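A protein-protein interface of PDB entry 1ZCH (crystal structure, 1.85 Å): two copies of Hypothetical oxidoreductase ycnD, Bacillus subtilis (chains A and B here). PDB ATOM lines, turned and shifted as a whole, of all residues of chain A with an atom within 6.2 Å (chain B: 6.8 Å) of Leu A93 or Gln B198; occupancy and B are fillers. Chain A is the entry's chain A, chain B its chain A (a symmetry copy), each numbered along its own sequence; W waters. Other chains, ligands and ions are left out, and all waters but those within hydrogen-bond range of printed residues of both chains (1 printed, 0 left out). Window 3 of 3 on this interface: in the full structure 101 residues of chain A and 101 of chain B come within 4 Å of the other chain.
A ring nitrogen (NE2) of His A94 is in hydrogen-bond range of the side-chain hydroxyl (OG) of Ser B221, 2.7 Å away.
N of Leu A93 sits at hydrogen-bond distance from O of Ile A88 (3.0 Å). The backbone carbonyl oxygen (O) of Ala A89 sits close to the backbone NH (N) of His A94 (3.4 Å). The side-chain amide oxygen (OD1) of Asn B219 lies close to the side-chain carboxylate (OD1) of Asp B201 (3.3 Å). The side-chain carboxylate of Asp B201 is in hydrogen-bond range of the backbone NH of Trp B220 (3.0 Å). OD2 of Asp B201 sits at hydrogen-bond distance from OG of Ser B221, 2.6 Å away. OD1 of Asn B219 lies within hydrogen-bond range of OG of Ser B221 (3.3 Å).
CD1 of Ile A88 touches CD2 of Leu B193 (3.9 Å). Thr B194 touches Ile A88. CD1 of Ile B197 touches CG2 of Ile A88, at 3.8 Å. CB of Ser B221 touches CB of Ala A89, 3.7 Å away. Ile B197 touches Leu A93 (CG2 to CD1, 3.7 Å). NE2 of Gln B198 touches CD2 of Leu A93 (3.9 Å). CD1 of Leu A93 touches OD2 of Asp B201, 3.9 Å away. Leu A93 touches Ser B221 (CD1 to CB, 3.9 Å).
Printed residues of chain B within 4 Å of Leu A93: Ile B197 (3.7 Å), Gln B198 (3.9 Å), Asp B201 (3.9 Å) and Ser B221 (3.9 Å). Of the printed residues of chain B, His A94 touches Ser B221. Printed residues of chain A within 4 Å of Leu B193: Ile A88. Printed residues of chain A within 4 Å of Ile B197: Ile A88 and Leu A93. Of the printed residues of chain A, Gln B198 touches Leu A93. Ala B199 touches none of the printed residues of chain A. Tyr B200 touches none of the printed residues of chain A. The nearest printed residue of chain A that does not touch Ile B197 is Ala A89 (5.0 Å).
No position is printed for both chains. Of the 9 pairs that touch across the chains among the printed residues, none has its exchanged pair printed and touching as well.
Water W1 lies within hydrogen-bond range of OG1 of Thr B194 (2.7 Å) and OD2 of Asp A92 (2.8 Å).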
ATOM      1  N   LYS A  87     -24.372 -27.814   9.117  1.00  0.00           N
ATOM      2  CA  LYS A  87     -24.063 -29.188   9.497  1.00  0.00           C
ATOM      3  C   LYS A  87     -23.441 -29.193  10.890  1.00  0.00           C
ATOM      4  O   LYS A  87     -23.799 -30.010  11.741  1.00  0.00           O
ATOM      5  CB  LYS A  87     -23.081 -29.820   8.511  1.00  0.00           C
ATOM      6  CG  LYS A  87     -22.741 -31.267   8.847  1.00  0.00           C
ATOM      7  CD  LYS A  87     -21.484 -31.717   8.132  1.00  0.00           C
ATOM      8  CE  LYS A  87     -20.358 -31.986   9.115  1.00  0.00           C
ATOM      9  NZ  LYS A  87     -20.665 -33.138  10.010  1.00  0.00           N
ATOM     10  N   ILE A  88     -22.497 -28.282  11.113  1.00  0.00           N
ATOM     11  CA  ILE A  88     -21.832 -28.179  12.409  1.00  0.00           C
ATOM     12  C   ILE A  88     -22.856 -27.876  13.496  1.00  0.00           C
ATOM     13  O   ILE A  88     -22.845 -28.490  14.569  1.00  0.00           O
ATOM     14  CB  ILE A  88     -20.770 -27.064  12.397  1.00  0.00           C
ATOM     15  CG1 ILE A  88     -19.625 -27.452  11.455  1.00  0.00           C
ATOM     16  CG2 ILE A  88     -20.265 -26.802  13.819  1.00  0.00           C
ATOM     17  CD1 ILE A  88     -18.619 -26.340  11.204  1.00  0.00           C
ATOM     18  N   ALA A  89     -23.742 -26.927  13.210  1.00  0.00           N
ATOM     19  CA  ALA A  89     -24.775 -26.538  14.164  1.00  0.00           C
ATOM     20  C   ALA A  89     -25.698 -27.695  14.540  1.00  0.00           C
ATOM     21  O   ALA A  89     -25.965 -27.928  15.717  1.00  0.00           O
ATOM     22  CB  ALA A  89     -25.598 -25.385  13.593  1.00  0.00           C
ATOM     23  N   LEU A  90     -26.194 -28.416  13.540  1.00  0.00           N
ATOM     24  CA  LEU A  90     -27.105 -29.525  13.812  1.00  0.00           C
ATOM     25  C   LEU A  90     -26.448 -30.786  14.351  1.00  0.00           C
ATOM     26  O   LEU A  90     -26.800 -31.269  15.429  1.00  0.00           O
ATOM     27  CB  LEU A  90     -27.904 -29.886  12.557  1.00  0.00           C
ATOM     28  CG  LEU A  90     -29.162 -29.054  12.282  1.00  0.00           C
ATOM     29  CD1 LEU A  90     -28.781 -27.627  11.903  1.00  0.00           C
ATOM     30  CD2 LEU A  90     -29.959 -29.711  11.174  1.00  0.00           C
ATOM     31  N   GLU A  91     -25.494 -31.312  13.596  1.00  0.00           N
ATOM     32  CA  GLU A  91     -24.824 -32.548  13.972  1.00  0.00           C
ATOM     33  C   GLU A  91     -23.843 -32.458  15.130  1.00  0.00           C
ATOM     34  O   GLU A  91     -23.893 -33.269  16.055  1.00  0.00           O
ATOM     35  CB  GLU A  91     -24.098 -33.130  12.756  1.00  0.00           C
ATOM     36  CG  GLU A  91     -25.006 -33.419  11.574  1.00  0.00           C
ATOM     37  CD  GLU A  91     -24.272 -34.111  10.441  1.00  0.00           C
ATOM     38  OE1 GLU A  91     -23.052 -34.351  10.572  1.00  0.00           O
ATOM     39  OE2 GLU A  91     -24.916 -34.413   9.418  1.00  0.00           O
ATOM     40  N   ASP A  92     -22.950 -31.478  15.080  1.00  0.00           N
ATOM     41  CA  ASP A  92     -21.937 -31.349  16.112  1.00  0.00           C
ATOM     42  C   ASP A  92     -22.348 -30.637  17.393  1.00  0.00           C
ATOM     43  O   ASP A  92     -21.931 -31.034  18.483  1.00  0.00           O
ATOM     44  CB  ASP A  92     -20.693 -30.677  15.524  1.00  0.00           C
ATOM     45  CG  ASP A  92     -20.203 -31.369  14.264  1.00  0.00           C
ATOM     46  OD1 ASP A  92     -20.483 -32.577  14.099  1.00  0.00           O
ATOM     47  OD2 ASP A  92     -19.529 -30.715  13.442  1.00  0.00           O
ATOM     48  N   LEU A  93     -23.168 -29.600  17.284  1.00  0.00           N
ATOM     49  CA  LEU A  93     -23.567 -28.863  18.477  1.00  0.00           C
ATOM     50  C   LEU A  93     -24.887 -29.296  19.111  1.00  0.00           C
ATOM     51  O   LEU A  93     -25.148 -28.974  20.270  1.00  0.00           O
ATOM     52  CB  LEU A  93     -23.618 -27.362  18.169  1.00  0.00           C
ATOM     53  CG  LEU A  93     -22.333 -26.733  17.613  1.00  0.00           C
ATOM     54  CD1 LEU A  93     -22.502 -25.216  17.525  1.00  0.00           C
ATOM     55  CD2 LEU A  93     -21.156 -27.078  18.513  1.00  0.00           C
ATOM     56  N   HIS A  94     -25.714 -30.027  18.372  1.00  0.00           N
ATOM     57  CA  HIS A  94     -27.003 -30.447  18.916  1.00  0.00           C
ATOM     58  C   HIS A  94     -27.395 -31.892  18.632  1.00  0.00           C
ATOM     59  O   HIS A  94     -28.512 -32.311  18.942  1.00  0.00           O
ATOM     60  CB  HIS A  94     -28.085 -29.488  18.420  1.00  0.00           C
ATOM     61  CG  HIS A  94     -27.862 -28.076  18.862  1.00  0.00           C
ATOM     62  ND1 HIS A  94     -28.017 -27.673  20.172  1.00  0.00           N
ATOM     63  CD2 HIS A  94     -27.415 -26.990  18.187  1.00  0.00           C
ATOM     64  CE1 HIS A  94     -27.673 -26.403  20.284  1.00  0.00           C
ATOM     65  NE2 HIS A  94     -27.303 -25.965  19.094  1.00  0.00           N
ATOM     66  N   ASP A  95     -26.467 -32.651  18.060  1.00  0.00           N
ATOM     67  CA  ASP A  95     -26.689 -34.059  17.745  1.00  0.00           C
ATOM     68  C   ASP A  95     -28.021 -34.319  17.048  1.00  0.00           C
ATOM     69  O   ASP A  95     -28.796 -35.189  17.452  1.00  0.00           O
ATOM     70  CB  ASP A  95     -26.593 -34.897  19.024  1.00  0.00           C
ATOM     71  CG  ASP A  95     -26.561 -36.389  18.742  1.00  0.00           C
ATOM     72  OD1 ASP A  95     -26.058 -36.784  17.666  1.00  0.00           O
ATOM     73  OD2 ASP A  95     -27.025 -37.169  19.603  1.00  0.00           O
ATOM     74  N   ASP B 191     -12.331 -27.120  12.703  1.00  0.00           N
ATOM     75  CA  ASP B 191     -12.191 -26.806  14.124  1.00  0.00           C
ATOM     76  C   ASP B 191     -12.355 -25.313  14.422  1.00  0.00           C
ATOM     77  O   ASP B 191     -13.102 -24.935  15.326  1.00  0.00           O
ATOM     78  CB  ASP B 191     -10.837 -27.299  14.649  1.00  0.00           C
ATOM     79  CG  ASP B 191      -9.664 -26.518  14.083  1.00  0.00           C
ATOM     80  OD1 ASP B 191      -9.547 -26.411  12.842  1.00  0.00           O
ATOM     81  OD2 ASP B 191      -8.848 -26.012  14.886  1.00  0.00           O
ATOM     82  N   LEU B 193     -13.749 -23.074  12.493  1.00  0.00           N
ATOM     83  CA  LEU B 193     -15.092 -22.683  12.085  1.00  0.00           C
ATOM     84  C   LEU B 193     -16.071 -22.988  13.212  1.00  0.00           C
ATOM     85  O   LEU B 193     -16.935 -22.177  13.537  1.00  0.00           O
ATOM     86  CB  LEU B 193     -15.486 -23.435  10.808  1.00  0.00           C
ATOM     87  CG  LEU B 193     -16.762 -23.025  10.069  1.00  0.00           C
ATOM     88  CD1 LEU B 193     -16.714 -21.542   9.707  1.00  0.00           C
ATOM     89  CD2 LEU B 193     -16.895 -23.868   8.805  1.00  0.00           C
ATOM     90  N   THR B 194     -15.922 -24.158  13.820  1.00  0.00           N
ATOM     91  CA  THR B 194     -16.795 -24.547  14.915  1.00  0.00           C
ATOM     92  C   THR B 194     -16.658 -23.559  16.076  1.00  0.00           C
ATOM     93  O   THR B 194     -17.656 -23.140  16.666  1.00  0.00           O
ATOM     94  CB  THR B 194     -16.461 -25.969  15.400  1.00  0.00           C
ATOM     95  OG1 THR B 194     -16.679 -26.895  14.326  1.00  0.00           O
ATOM     96  CG2 THR B 194     -17.338 -26.352  16.583  1.00  0.00           C
ATOM     97  N   SER B 195     -15.423 -23.181  16.392  1.00  0.00           N
ATOM     98  CA  SER B 195     -15.176 -22.234  17.477  1.00  0.00           C
ATOM     99  C   SER B 195     -15.879 -20.901  17.233  1.00  0.00           C
ATOM    100  O   SER B 195     -16.430 -20.310  18.162  1.00  0.00           O
ATOM    101  CB  SER B 195     -13.672 -21.998  17.653  1.00  0.00           C
ATOM    102  OG  SER B 195     -13.031 -23.186  18.078  1.00  0.00           O
ATOM    103  N   HIS B 196     -15.857 -20.424  15.990  1.00  0.00           N
ATOM    104  CA  HIS B 196     -16.518 -19.162  15.659  1.00  0.00           C
ATOM    105  C   HIS B 196     -18.023 -19.269  15.870  1.00  0.00           C
ATOM    106  O   HIS B 196     -18.661 -18.323  16.338  1.00  0.00           O
ATOM    107  CB  HIS B 196     -16.253 -18.769  14.204  1.00  0.00           C
ATOM    108  CG  HIS B 196     -14.875 -18.237  13.961  1.00  0.00           C
ATOM    109  ND1 HIS B 196     -14.373 -17.143  14.631  1.00  0.00           N
ATOM    110  CD2 HIS B 196     -13.902 -18.639  13.111  1.00  0.00           C
ATOM    111  CE1 HIS B 196     -13.147 -16.893  14.204  1.00  0.00           C
ATOM    112  NE2 HIS B 196     -12.837 -17.787  13.282  1.00  0.00           N
ATOM    113  N   ILE B 197     -18.591 -20.417  15.508  1.00  0.00           N
ATOM    114  CA  ILE B 197     -20.024 -20.627  15.671  1.00  0.00           C
ATOM    115  C   ILE B 197     -20.410 -20.634  17.153  1.00  0.00           C
ATOM    116  O   ILE B 197     -21.427 -20.055  17.542  1.00  0.00           O
ATOM    117  CB  ILE B 197     -20.473 -21.950  15.006  1.00  0.00           C
ATOM    118  CG1 ILE B 197     -20.273 -21.858  13.488  1.00  0.00           C
ATOM    119  CG2 ILE B 197     -21.938 -22.230  15.328  1.00  0.00           C
ATOM    120  CD1 ILE B 197     -20.583 -23.144  12.738  1.00  0.00           C
ATOM    121  N   GLN B 198     -19.596 -21.279  17.982  1.00  0.00           N
ATOM    122  CA  GLN B 198     -19.881 -21.327  19.413  1.00  0.00           C
ATOM    123  C   GLN B 198     -19.787 -19.936  20.044  1.00  0.00           C
ATOM    124  O   GLN B 198     -20.565 -19.600  20.938  1.00  0.00           O
ATOM    125  CB  GLN B 198     -18.931 -22.306  20.110  1.00  0.00           C
ATOM    126  CG  GLN B 198     -19.209 -23.757  19.729  1.00  0.00           C
ATOM    127  CD  GLN B 198     -18.229 -24.732  20.343  1.00  0.00           C
ATOM    128  OE1 GLN B 198     -17.026 -24.664  20.088  1.00  0.00           O
ATOM    129  NE2 GLN B 198     -18.740 -25.654  21.156  1.00  0.00           N
ATOM    130  N   ALA B 199     -18.842 -19.125  19.576  1.00  0.00           N
ATOM    131  CA  ALA B 199     -18.697 -17.767  20.099  1.00  0.00           C
ATOM    132  C   ALA B 199     -19.910 -16.956  19.652  1.00  0.00           C
ATOM    133  O   ALA B 199     -20.463 -16.164  20.416  1.00  0.00           O
ATOM    134  CB  ALA B 199     -17.414 -17.133  19.575  1.00  0.00           C
ATOM    135  N   TYR B 200     -20.320 -17.164  18.406  1.00  0.00           N
ATOM    136  CA  TYR B 200     -21.475 -16.466  17.849  1.00  0.00           C
ATOM    137  C   TYR B 200     -22.722 -16.809  18.658  1.00  0.00           C
ATOM    138  O   TYR B 200     -23.555 -15.939  18.926  1.00  0.00           O
ATOM    139  CB  TYR B 200     -21.664 -16.871  16.382  1.00  0.00           C
ATOM    140  CG  TYR B 200     -22.819 -16.193  15.667  1.00  0.00           C
ATOM    141  CD1 TYR B 200     -23.013 -14.811  15.749  1.00  0.00           C
ATOM    142  CD2 TYR B 200     -23.685 -16.928  14.863  1.00  0.00           C
ATOM    143  CE1 TYR B 200     -24.043 -14.183  15.042  1.00  0.00           C
ATOM    144  CE2 TYR B 200     -24.714 -16.312  14.148  1.00  0.00           C
ATOM    145  CZ  TYR B 200     -24.888 -14.941  14.239  1.00  0.00           C
ATOM    146  OH  TYR B 200     -25.895 -14.332  13.519  1.00  0.00           O
ATOM    147  N   ASP B 201     -22.847 -18.074  19.054  1.00  0.00           N
ATOM    148  CA  ASP B 201     -24.006 -18.509  19.838  1.00  0.00           C
ATOM    149  C   ASP B 201     -24.151 -17.710  21.132  1.00  0.00           C
ATOM    150  O   ASP B 201     -25.252 -17.278  21.482  1.00  0.00           O
ATOM    151  CB  ASP B 201     -23.919 -20.006  20.178  1.00  0.00           C
ATOM    152  CG  ASP B 201     -24.540 -20.892  19.106  1.00  0.00           C
ATOM    153  OD1 ASP B 201     -25.388 -20.395  18.334  1.00  0.00           O
ATOM    154  OD2 ASP B 201     -24.195 -22.094  19.046  1.00  0.00           O
ATOM    155  N   GLU B 202     -23.045 -17.512  21.840  1.00  0.00           N
ATOM    156  CA  GLU B 202     -23.092 -16.760  23.091  1.00  0.00           C
ATOM    157  C   GLU B 202     -23.534 -15.335  22.806  1.00  0.00           C
ATOM    158  O   GLU B 202     -24.343 -14.765  23.537  1.00  0.00           O
ATOM    159  CB  GLU B 202     -21.722 -16.746  23.769  1.00  0.00           C
ATOM    160  CG  GLU B 202     -21.075 -18.114  23.872  1.00  0.00           C
ATOM    161  CD  GLU B 202     -20.147 -18.226  25.061  1.00  0.00           C
ATOM    162  OE1 GLU B 202     -19.420 -17.247  25.343  1.00  0.00           O
ATOM    163  OE2 GLU B 202     -20.141 -19.297  25.708  1.00  0.00           O
ATOM    164  N   GLN B 203     -23.002 -14.766  21.731  1.00  0.00           N
ATOM    165  CA  GLN B 203     -23.351 -13.408  21.336  1.00  0.00           C
ATOM    166  C   GLN B 203     -24.839 -13.304  21.024  1.00  0.00           C
ATOM    167  O   GLN B 203     -25.506 -12.353  21.438  1.00  0.00           O
ATOM    168  CB  GLN B 203     -22.559 -13.002  20.091  1.00  0.00           C
ATOM    169  CG  GLN B 203     -21.060 -12.903  20.282  1.00  0.00           C
ATOM    170  CD  GLN B 203     -20.336 -12.636  18.975  1.00  0.00           C
ATOM    171  OE1 GLN B 203     -20.689 -11.717  18.237  1.00  0.00           O
ATOM    172  NE2 GLN B 203     -19.319 -13.439  18.684  1.00  0.00           N
ATOM    173  N   ASN B 219     -30.120 -19.380  20.968  1.00  0.00           N
ATOM    174  CA  ASN B 219     -28.957 -18.892  20.231  1.00  0.00           C
ATOM    175  C   ASN B 219     -29.112 -19.210  18.745  1.00  0.00           C
ATOM    176  O   ASN B 219     -30.193 -19.599  18.299  1.00  0.00           O
ATOM    177  CB  ASN B 219     -27.647 -19.479  20.779  1.00  0.00           C
ATOM    178  CG  ASN B 219     -27.606 -20.988  20.725  1.00  0.00           C
ATOM    179  OD1 ASN B 219     -28.132 -21.604  19.802  1.00  0.00           O
ATOM    180  ND2 ASN B 219     -26.955 -21.598  21.714  1.00  0.00           N
ATOM    181  N   TRP B 220     -28.039 -19.042  17.978  1.00  0.00           N
ATOM    182  CA  TRP B 220     -28.094 -19.283  16.540  1.00  0.00           C
ATOM    183  C   TRP B 220     -28.197 -20.759  16.155  1.00  0.00           C
ATOM    184  O   TRP B 220     -29.131 -21.157  15.463  1.00  0.00           O
ATOM    185  CB  TRP B 220     -26.869 -18.661  15.862  1.00  0.00           C
ATOM    186  CG  TRP B 220     -26.903 -18.723  14.365  1.00  0.00           C
ATOM    187  CD1 TRP B 220     -27.679 -17.970  13.526  1.00  0.00           C
ATOM    188  CD2 TRP B 220     -26.100 -19.560  13.526  1.00  0.00           C
ATOM    189  NE1 TRP B 220     -27.402 -18.283  12.216  1.00  0.00           N
ATOM    190  CE2 TRP B 220     -26.436 -19.255  12.186  1.00  0.00           C
ATOM    191  CE3 TRP B 220     -25.127 -20.539  13.774  1.00  0.00           C
ATOM    192  CZ2 TRP B 220     -25.833 -19.895  11.096  1.00  0.00           C
ATOM    193  CZ3 TRP B 220     -24.525 -21.180  12.689  1.00  0.00           C
ATOM    194  CH2 TRP B 220     -24.882 -20.850  11.365  1.00  0.00           C
ATOM    195  N   SER B 221     -27.242 -21.577  16.593  1.00  0.00           N
ATOM    196  CA  SER B 221     -27.280 -22.993  16.241  1.00  0.00           C
ATOM    197  C   SER B 221     -28.596 -23.656  16.665  1.00  0.00           C
ATOM    198  O   SER B 221     -29.104 -24.536  15.966  1.00  0.00           O
ATOM    199  CB  SER B 221     -26.085 -23.738  16.855  1.00  0.00           C
ATOM    200  OG  SER B 221     -26.117 -23.697  18.270  1.00  0.00           O
HETATM  201  O   HOH W   1     -17.375 -29.456  14.628  1.00  0.00           O
